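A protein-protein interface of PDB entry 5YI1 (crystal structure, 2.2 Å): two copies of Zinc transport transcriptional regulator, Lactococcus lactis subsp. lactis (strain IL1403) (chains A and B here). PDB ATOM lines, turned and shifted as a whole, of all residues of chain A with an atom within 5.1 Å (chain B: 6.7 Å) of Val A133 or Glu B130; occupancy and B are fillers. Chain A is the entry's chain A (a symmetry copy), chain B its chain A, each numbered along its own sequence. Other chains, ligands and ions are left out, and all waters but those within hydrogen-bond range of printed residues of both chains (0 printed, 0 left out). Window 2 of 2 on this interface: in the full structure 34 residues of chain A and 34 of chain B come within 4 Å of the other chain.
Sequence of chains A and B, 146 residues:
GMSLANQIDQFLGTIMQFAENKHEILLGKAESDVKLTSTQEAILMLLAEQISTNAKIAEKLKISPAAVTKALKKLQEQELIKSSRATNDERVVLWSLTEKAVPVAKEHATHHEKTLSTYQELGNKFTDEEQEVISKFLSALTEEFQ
NE2 of Gln B131 lies within hydrogen-bond range of O of Phe B126. The backbone NH (N) of Thr B127 is in hydrogen-bond range of the side-chain carboxylate (OE1) of Glu B130 (2.9 Å).
Among the printed residues, merely in contact across the chains: Glu A130 with Val B133 (3.8 Å), Val A133 with Phe B126 (3.9 Å), Val A133 with Glu B130 (3.8 Å), Val A133 with Ile B134 (3.98 Å), Ile A134 with Val B133 (3.98 Å), Phe A137 with Phe B126 (3.7 Å) and Phe A137 with Ile B134 (3.9 Å).
Glu A129 touches none of the printed residues of chain B. Printed residues of chain B within 4 Å of Glu A130: Val B133 (3.8 Å). Of the printed residues of chain B, Val A133 touches Phe B126, Glu B130 and Ile B134. Of the printed residues of chain B, Ile A134 touches Val B133. Of the printed residues of chain B, Phe A137 touches Phe B126 and Ile B134. Of the printed residues of chain A, Glu B130 touches Val A133. Of the printed residues of chain A, Val B133 touches Glu A130 (3.8 Å) and Ile A134 (3.98 Å). The nearest printed residue of chain A that does not touch Glu B130 is Lys A136 (6.5 Å).
Hydrophobic or aromatic side chains of chain B within 4 Å of the printed part of chain A: Phe B126, Val B133 and Ile B134. Hydrophobic or aromatic side chains of chain A that line the printed part of chain B: Val A133, Ile A134 and Phe A137. Among the printed residues, 7 pairs touch across the chains.
Glu A130 touches Val B133, and with the chains exchanged Val A133 touches Glu B130. Val A133 touches Ile B134, and with the chains exchanged Ile A134 touches Val B133. Positions printed for both chains: 129, 130, 131, 132, 133, 134 and 135. Of the 7 pairs that touch across the chains among the printed residues, 4 have their exchanged pair printed and touching as well.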
ATOM      1  N   GLU A 129       7.022  14.515  15.539  1.00  0.00           N
ATOM      2  CA  GLU A 129       7.019  14.862  14.124  1.00  0.00           C
ATOM      3  C   GLU A 129       5.912  15.865  13.804  1.00  0.00           C
ATOM      4  O   GLU A 129       6.113  16.795  13.024  1.00  0.00           O
ATOM      5  CB  GLU A 129       6.868  13.602  13.280  1.00  0.00           C
ATOM      6  CG  GLU A 129       6.452  13.827  11.845  1.00  0.00           C
ATOM      7  CD  GLU A 129       6.227  12.500  11.119  1.00  0.00           C
ATOM      8  OE1 GLU A 129       5.054  12.074  10.952  1.00  0.00           O
ATOM      9  OE2 GLU A 129       7.242  11.867  10.754  1.00  0.00           O
ATOM     10  N   GLU A 130       4.747  15.674  14.415  1.00  0.00           N
ATOM     11  CA  GLU A 130       3.619  16.588  14.219  1.00  0.00           C
ATOM     12  C   GLU A 130       3.947  17.951  14.836  1.00  0.00           C
ATOM     13  O   GLU A 130       3.684  19.010  14.244  1.00  0.00           O
ATOM     14  CB  GLU A 130       2.344  15.981  14.823  1.00  0.00           C
ATOM     15  CG  GLU A 130       1.829  14.780  13.984  1.00  0.00           C
ATOM     16  CD  GLU A 130       0.798  13.938  14.716  1.00  0.00           C
ATOM     17  OE1 GLU A 130       0.646  14.107  15.948  1.00  0.00           O
ATOM     18  OE2 GLU A 130       0.155  13.085  14.067  1.00  0.00           O
ATOM     19  N   GLN A 131       4.545  17.915  16.020  1.00  0.00           N
ATOM     20  CA  GLN A 131       4.988  19.141  16.691  1.00  0.00           C
ATOM     21  C   GLN A 131       5.981  19.950  15.864  1.00  0.00           C
ATOM     22  O   GLN A 131       5.996  21.164  15.940  1.00  0.00           O
ATOM     23  CB  GLN A 131       5.599  18.833  18.047  1.00  0.00           C
ATOM     24  CG  GLN A 131       4.631  18.300  19.063  1.00  0.00           C
ATOM     25  CD  GLN A 131       5.268  18.241  20.424  1.00  0.00           C
ATOM     26  OE1 GLN A 131       6.272  18.896  20.654  1.00  0.00           O
ATOM     27  NE2 GLN A 131       4.700  17.454  21.327  1.00  0.00           N
ATOM     28  N   GLU A 132       6.809  19.269  15.078  1.00  0.00           N
ATOM     29  CA  GLU A 132       7.750  19.946  14.198  1.00  0.00           C
ATOM     30  C   GLU A 132       7.008  20.654  13.072  1.00  0.00           C
ATOM     31  O   GLU A 132       7.374  21.737  12.645  1.00  0.00           O
ATOM     32  CB  GLU A 132       8.722  18.927  13.603  1.00  0.00           C
ATOM     33  CG  GLU A 132       9.756  19.525  12.656  1.00  0.00           C
ATOM     34  CD  GLU A 132      10.984  20.077  13.378  1.00  0.00           C
ATOM     35  OE1 GLU A 132      12.024  20.281  12.705  1.00  0.00           O
ATOM     36  OE2 GLU A 132      10.917  20.309  14.611  1.00  0.00           O
ATOM     37  N   VAL A 133       5.974  20.010  12.570  1.00  0.00           N
ATOM     38  CA  VAL A 133       5.137  20.612  11.551  1.00  0.00           C
ATOM     39  C   VAL A 133       4.524  21.890  12.120  1.00  0.00           C
ATOM     40  O   VAL A 133       4.627  22.950  11.526  1.00  0.00           O
ATOM     41  CB  VAL A 133       4.041  19.616  11.097  1.00  0.00           C
ATOM     42  CG1 VAL A 133       2.963  20.312  10.227  1.00  0.00           C
ATOM     43  CG2 VAL A 133       4.694  18.418  10.388  1.00  0.00           C
ATOM     44  N   ILE A 134       3.924  21.775  13.297  1.00  0.00           N
ATOM     45  CA  ILE A 134       3.299  22.916  13.965  1.00  0.00           C
ATOM     46  C   ILE A 134       4.310  24.028  14.272  1.00  0.00           C
ATOM     47  O   ILE A 134       4.016  25.215  14.091  1.00  0.00           O
ATOM     48  CB  ILE A 134       2.620  22.488  15.295  1.00  0.00           C
ATOM     49  CG1 ILE A 134       1.385  21.610  15.018  1.00  0.00           C
ATOM     50  CG2 ILE A 134       2.262  23.727  16.133  1.00  0.00           C
ATOM     51  CD1 ILE A 134       1.049  20.654  16.181  1.00  0.00           C
ATOM     52  N   SER A 135       5.495  23.639  14.752  1.00  0.00           N
ATOM     53  CA  SER A 135       6.545  24.616  15.042  1.00  0.00           C
ATOM     54  C   SER A 135       6.930  25.403  13.787  1.00  0.00           C
ATOM     55  O   SER A 135       6.970  26.623  13.804  1.00  0.00           O
ATOM     56  CB  SER A 135       7.788  23.919  15.627  1.00  0.00           C
ATOM     57  OG  SER A 135       8.787  24.874  15.925  1.00  0.00           O
ATOM     58  N   LYS A 136       7.218  24.705  12.695  1.00  0.00           N
ATOM     59  CA  LYS A 136       7.569  25.400  11.452  1.00  0.00           C
ATOM     60  C   LYS A 136       6.428  26.307  10.989  1.00  0.00           C
ATOM     61  O   LYS A 136       6.655  27.419  10.515  1.00  0.00           O
ATOM     62  CB  LYS A 136       7.915  24.412  10.329  1.00  0.00           C
ATOM     63  CG  LYS A 136       9.114  23.477  10.597  1.00  0.00           C
ATOM     64  CD  LYS A 136       9.485  22.719   9.308  1.00  0.00           C
ATOM     65  CE  LYS A 136      10.328  21.478   9.553  1.00  0.00           C
ATOM     66  NZ  LYS A 136      10.634  20.754   8.278  1.00  0.00           N
ATOM     67  N   PHE A 137       5.198  25.816  11.103  1.00  0.00           N
ATOM     68  CA  PHE A 137       4.060  26.603  10.666  1.00  0.00           C
ATOM     69  C   PHE A 137       4.016  27.911  11.453  1.00  0.00           C
ATOM     70  O   PHE A 137       3.928  28.996  10.877  1.00  0.00           O
ATOM     71  CB  PHE A 137       2.760  25.816  10.851  1.00  0.00           C
ATOM     72  CG  PHE A 137       1.536  26.646  10.662  1.00  0.00           C
ATOM     73  CD1 PHE A 137       1.125  27.005   9.389  1.00  0.00           C
ATOM     74  CD2 PHE A 137       0.820  27.116  11.759  1.00  0.00           C
ATOM     75  CE1 PHE A 137      -0.012  27.797   9.202  1.00  0.00           C
ATOM     76  CE2 PHE A 137      -0.307  27.885  11.584  1.00  0.00           C
ATOM     77  CZ  PHE A 137      -0.721  28.231  10.292  1.00  0.00           C
ATOM     78  N   LEU A 138       4.081  27.796  12.778  1.00  0.00           N
ATOM     79  CA  LEU A 138       3.997  28.967  13.650  1.00  0.00           C
ATOM     80  C   LEU A 138       5.148  29.950  13.423  1.00  0.00           C
ATOM     81  O   LEU A 138       4.927  31.158  13.423  1.00  0.00           O
ATOM     82  CB  LEU A 138       3.919  28.564  15.129  1.00  0.00           C
ATOM     83  CG  LEU A 138       2.659  27.856  15.658  1.00  0.00           C
ATOM     84  CD1 LEU A 138       2.776  27.579  17.145  1.00  0.00           C
ATOM     85  CD2 LEU A 138       1.399  28.638  15.363  1.00  0.00           C
ATOM     86  N   LYS B 125       3.063  25.196   1.436  1.00  0.00           N
ATOM     87  CA  LYS B 125       4.379  24.632   1.730  1.00  0.00           C
ATOM     88  C   LYS B 125       4.263  23.319   2.496  1.00  0.00           C
ATOM     89  O   LYS B 125       5.257  22.657   2.758  1.00  0.00           O
ATOM     90  CB  LYS B 125       5.222  25.630   2.520  1.00  0.00           C
ATOM     91  CG  LYS B 125       5.505  26.912   1.750  1.00  0.00           C
ATOM     92  CD  LYS B 125       6.275  27.904   2.606  1.00  0.00           C
ATOM     93  CE  LYS B 125       6.569  29.200   1.838  1.00  0.00           C
ATOM     94  NZ  LYS B 125       7.203  30.219   2.741  1.00  0.00           N
ATOM     95  N   PHE B 126       3.036  22.958   2.857  1.00  0.00           N
ATOM     96  CA  PHE B 126       2.762  21.758   3.631  1.00  0.00           C
ATOM     97  C   PHE B 126       1.890  20.764   2.834  1.00  0.00           C
ATOM     98  O   PHE B 126       0.963  21.154   2.124  1.00  0.00           O
ATOM     99  CB  PHE B 126       2.055  22.122   4.940  1.00  0.00           C
ATOM    100  CG  PHE B 126       2.864  23.021   5.849  1.00  0.00           C
ATOM    101  CD1 PHE B 126       3.712  22.472   6.813  1.00  0.00           C
ATOM    102  CD2 PHE B 126       2.767  24.402   5.750  1.00  0.00           C
ATOM    103  CE1 PHE B 126       4.467  23.299   7.672  1.00  0.00           C
ATOM    104  CE2 PHE B 126       3.515  25.247   6.604  1.00  0.00           C
ATOM    105  CZ  PHE B 126       4.369  24.685   7.557  1.00  0.00           C
ATOM    106  N   THR B 127       2.182  19.483   2.978  1.00  0.00           N
ATOM    107  CA  THR B 127       1.351  18.436   2.397  1.00  0.00           C
ATOM    108  C   THR B 127      -0.016  18.453   3.055  1.00  0.00           C
ATOM    109  O   THR B 127      -0.185  19.002   4.150  1.00  0.00           O
ATOM    110  CB  THR B 127       1.959  17.031   2.642  1.00  0.00           C
ATOM    111  OG1 THR B 127       2.104  16.818   4.054  1.00  0.00           O
ATOM    112  CG2 THR B 127       3.311  16.891   1.946  1.00  0.00           C
ATOM    113  N   ASP B 128      -0.990  17.843   2.388  1.00  0.00           N
ATOM    114  CA  ASP B 128      -2.326  17.667   2.941  1.00  0.00           C
ATOM    115  C   ASP B 128      -2.291  17.070   4.343  1.00  0.00           C
ATOM    116  O   ASP B 128      -3.027  17.494   5.232  1.00  0.00           O
ATOM    117  CB  ASP B 128      -3.141  16.757   2.013  1.00  0.00           C
ATOM    118  CG  ASP B 128      -3.364  17.378   0.646  1.00  0.00           C
ATOM    119  OD1 ASP B 128      -3.545  18.624   0.567  1.00  0.00           O
ATOM    120  OD2 ASP B 128      -3.350  16.626  -0.350  1.00  0.00           O
ATOM    121  N   GLU B 129      -1.440  16.073   4.540  1.00  0.00           N
ATOM    122  CA  GLU B 129      -1.348  15.432   5.845  1.00  0.00           C
ATOM    123  C   GLU B 129      -0.838  16.407   6.904  1.00  0.00           C
ATOM    124  O   GLU B 129      -1.322  16.417   8.035  1.00  0.00           O
ATOM    125  CB  GLU B 129      -0.448  14.205   5.761  1.00  0.00           C
ATOM    126  CG  GLU B 129       0.060  13.679   7.082  1.00  0.00           C
ATOM    127  CD  GLU B 129       1.034  12.518   6.879  1.00  0.00           C
ATOM    128  OE1 GLU B 129       2.273  12.725   6.965  1.00  0.00           O
ATOM    129  OE2 GLU B 129       0.546  11.403   6.591  1.00  0.00           O
ATOM    130  N   GLU B 130       0.138  17.230   6.529  1.00  0.00           N
ATOM    131  CA  GLU B 130       0.687  18.236   7.442  1.00  0.00           C
ATOM    132  C   GLU B 130      -0.374  19.302   7.733  1.00  0.00           C
ATOM    133  O   GLU B 130      -0.560  19.734   8.881  1.00  0.00           O
ATOM    134  CB  GLU B 130       1.961  18.847   6.840  1.00  0.00           C
ATOM    135  CG  GLU B 130       3.141  17.839   6.854  1.00  0.00           C
ATOM    136  CD  GLU B 130       4.299  18.262   5.965  1.00  0.00           C
ATOM    137  OE1 GLU B 130       4.120  19.190   5.143  1.00  0.00           O
ATOM    138  OE2 GLU B 130       5.383  17.649   6.067  1.00  0.00           O
ATOM    139  N   GLN B 131      -1.083  19.705   6.685  1.00  0.00           N
ATOM    140  CA  GLN B 131      -2.184  20.662   6.830  1.00  0.00           C
ATOM    141  C   GLN B 131      -3.275  20.180   7.779  1.00  0.00           C
ATOM    142  O   GLN B 131      -3.896  20.978   8.454  1.00  0.00           O
ATOM    143  CB  GLN B 131      -2.801  20.994   5.482  1.00  0.00           C
ATOM    144  CG  GLN B 131      -1.902  21.751   4.551  1.00  0.00           C
ATOM    145  CD  GLN B 131      -2.664  22.229   3.346  1.00  0.00           C
ATOM    146  OE1 GLN B 131      -3.883  22.286   3.382  1.00  0.00           O
ATOM    147  NE2 GLN B 131      -1.960  22.563   2.274  1.00  0.00           N
ATOM    148  N   GLU B 132      -3.503  18.871   7.822  1.00  0.00           N
ATOM    149  CA  GLU B 132      -4.475  18.299   8.741  1.00  0.00           C
ATOM    150  C   GLU B 132      -3.984  18.421  10.177  1.00  0.00           C
ATOM    151  O   GLU B 132      -4.749  18.660  11.098  1.00  0.00           O
ATOM    152  CB  GLU B 132      -4.696  16.824   8.405  1.00  0.00           C
ATOM    153  CG  GLU B 132      -5.697  16.116   9.311  1.00  0.00           C
ATOM    154  CD  GLU B 132      -7.146  16.298   8.862  1.00  0.00           C
ATOM    155  OE1 GLU B 132      -8.009  15.508   9.316  1.00  0.00           O
ATOM    156  OE2 GLU B 132      -7.429  17.225   8.062  1.00  0.00           O
ATOM    157  N   VAL B 133      -2.695  18.220  10.364  1.00  0.00           N
ATOM    158  CA  VAL B 133      -2.090  18.389  11.671  1.00  0.00           C
ATOM    159  C   VAL B 133      -2.298  19.834  12.119  1.00  0.00           C
ATOM    160  O   VAL B 133      -2.797  20.086  13.203  1.00  0.00           O
ATOM    161  CB  VAL B 133      -0.585  18.027  11.617  1.00  0.00           C
ATOM    162  CG1 VAL B 133       0.152  18.462  12.910  1.00  0.00           C
ATOM    163  CG2 VAL B 133      -0.425  16.527  11.319  1.00  0.00           C
ATOM    164  N   ILE B 134      -1.946  20.771  11.249  1.00  0.00           N
ATOM    165  CA  ILE B 134      -2.095  22.196  11.539  1.00  0.00           C
ATOM    166  C   ILE B 134      -3.558  22.582  11.792  1.00  0.00           C
ATOM    167  O   ILE B 134      -3.855  23.359  12.707  1.00  0.00           O
ATOM    168  CB  ILE B 134      -1.550  23.069  10.375  1.00  0.00           C
ATOM    169  CG1 ILE B 134      -0.016  22.956  10.282  1.00  0.00           C
ATOM    170  CG2 ILE B 134      -2.005  24.528  10.545  1.00  0.00           C
ATOM    171  CD1 ILE B 134       0.526  23.229   8.864  1.00  0.00           C
ATOM    172  N   SER B 135      -4.465  22.050  10.968  1.00  0.00           N
ATOM    173  CA  SER B 135      -5.891  22.323  11.144  1.00  0.00           C
ATOM    174  C   SER B 135      -6.375  21.864  12.522  1.00  0.00           C
ATOM    175  O   SER B 135      -7.011  22.618  13.242  1.00  0.00           O
ATOM    176  CB  SER B 135      -6.716  21.633  10.041  1.00  0.00           C
ATOM    177  OG  SER B 135      -8.090  21.922  10.208  1.00  0.00           O
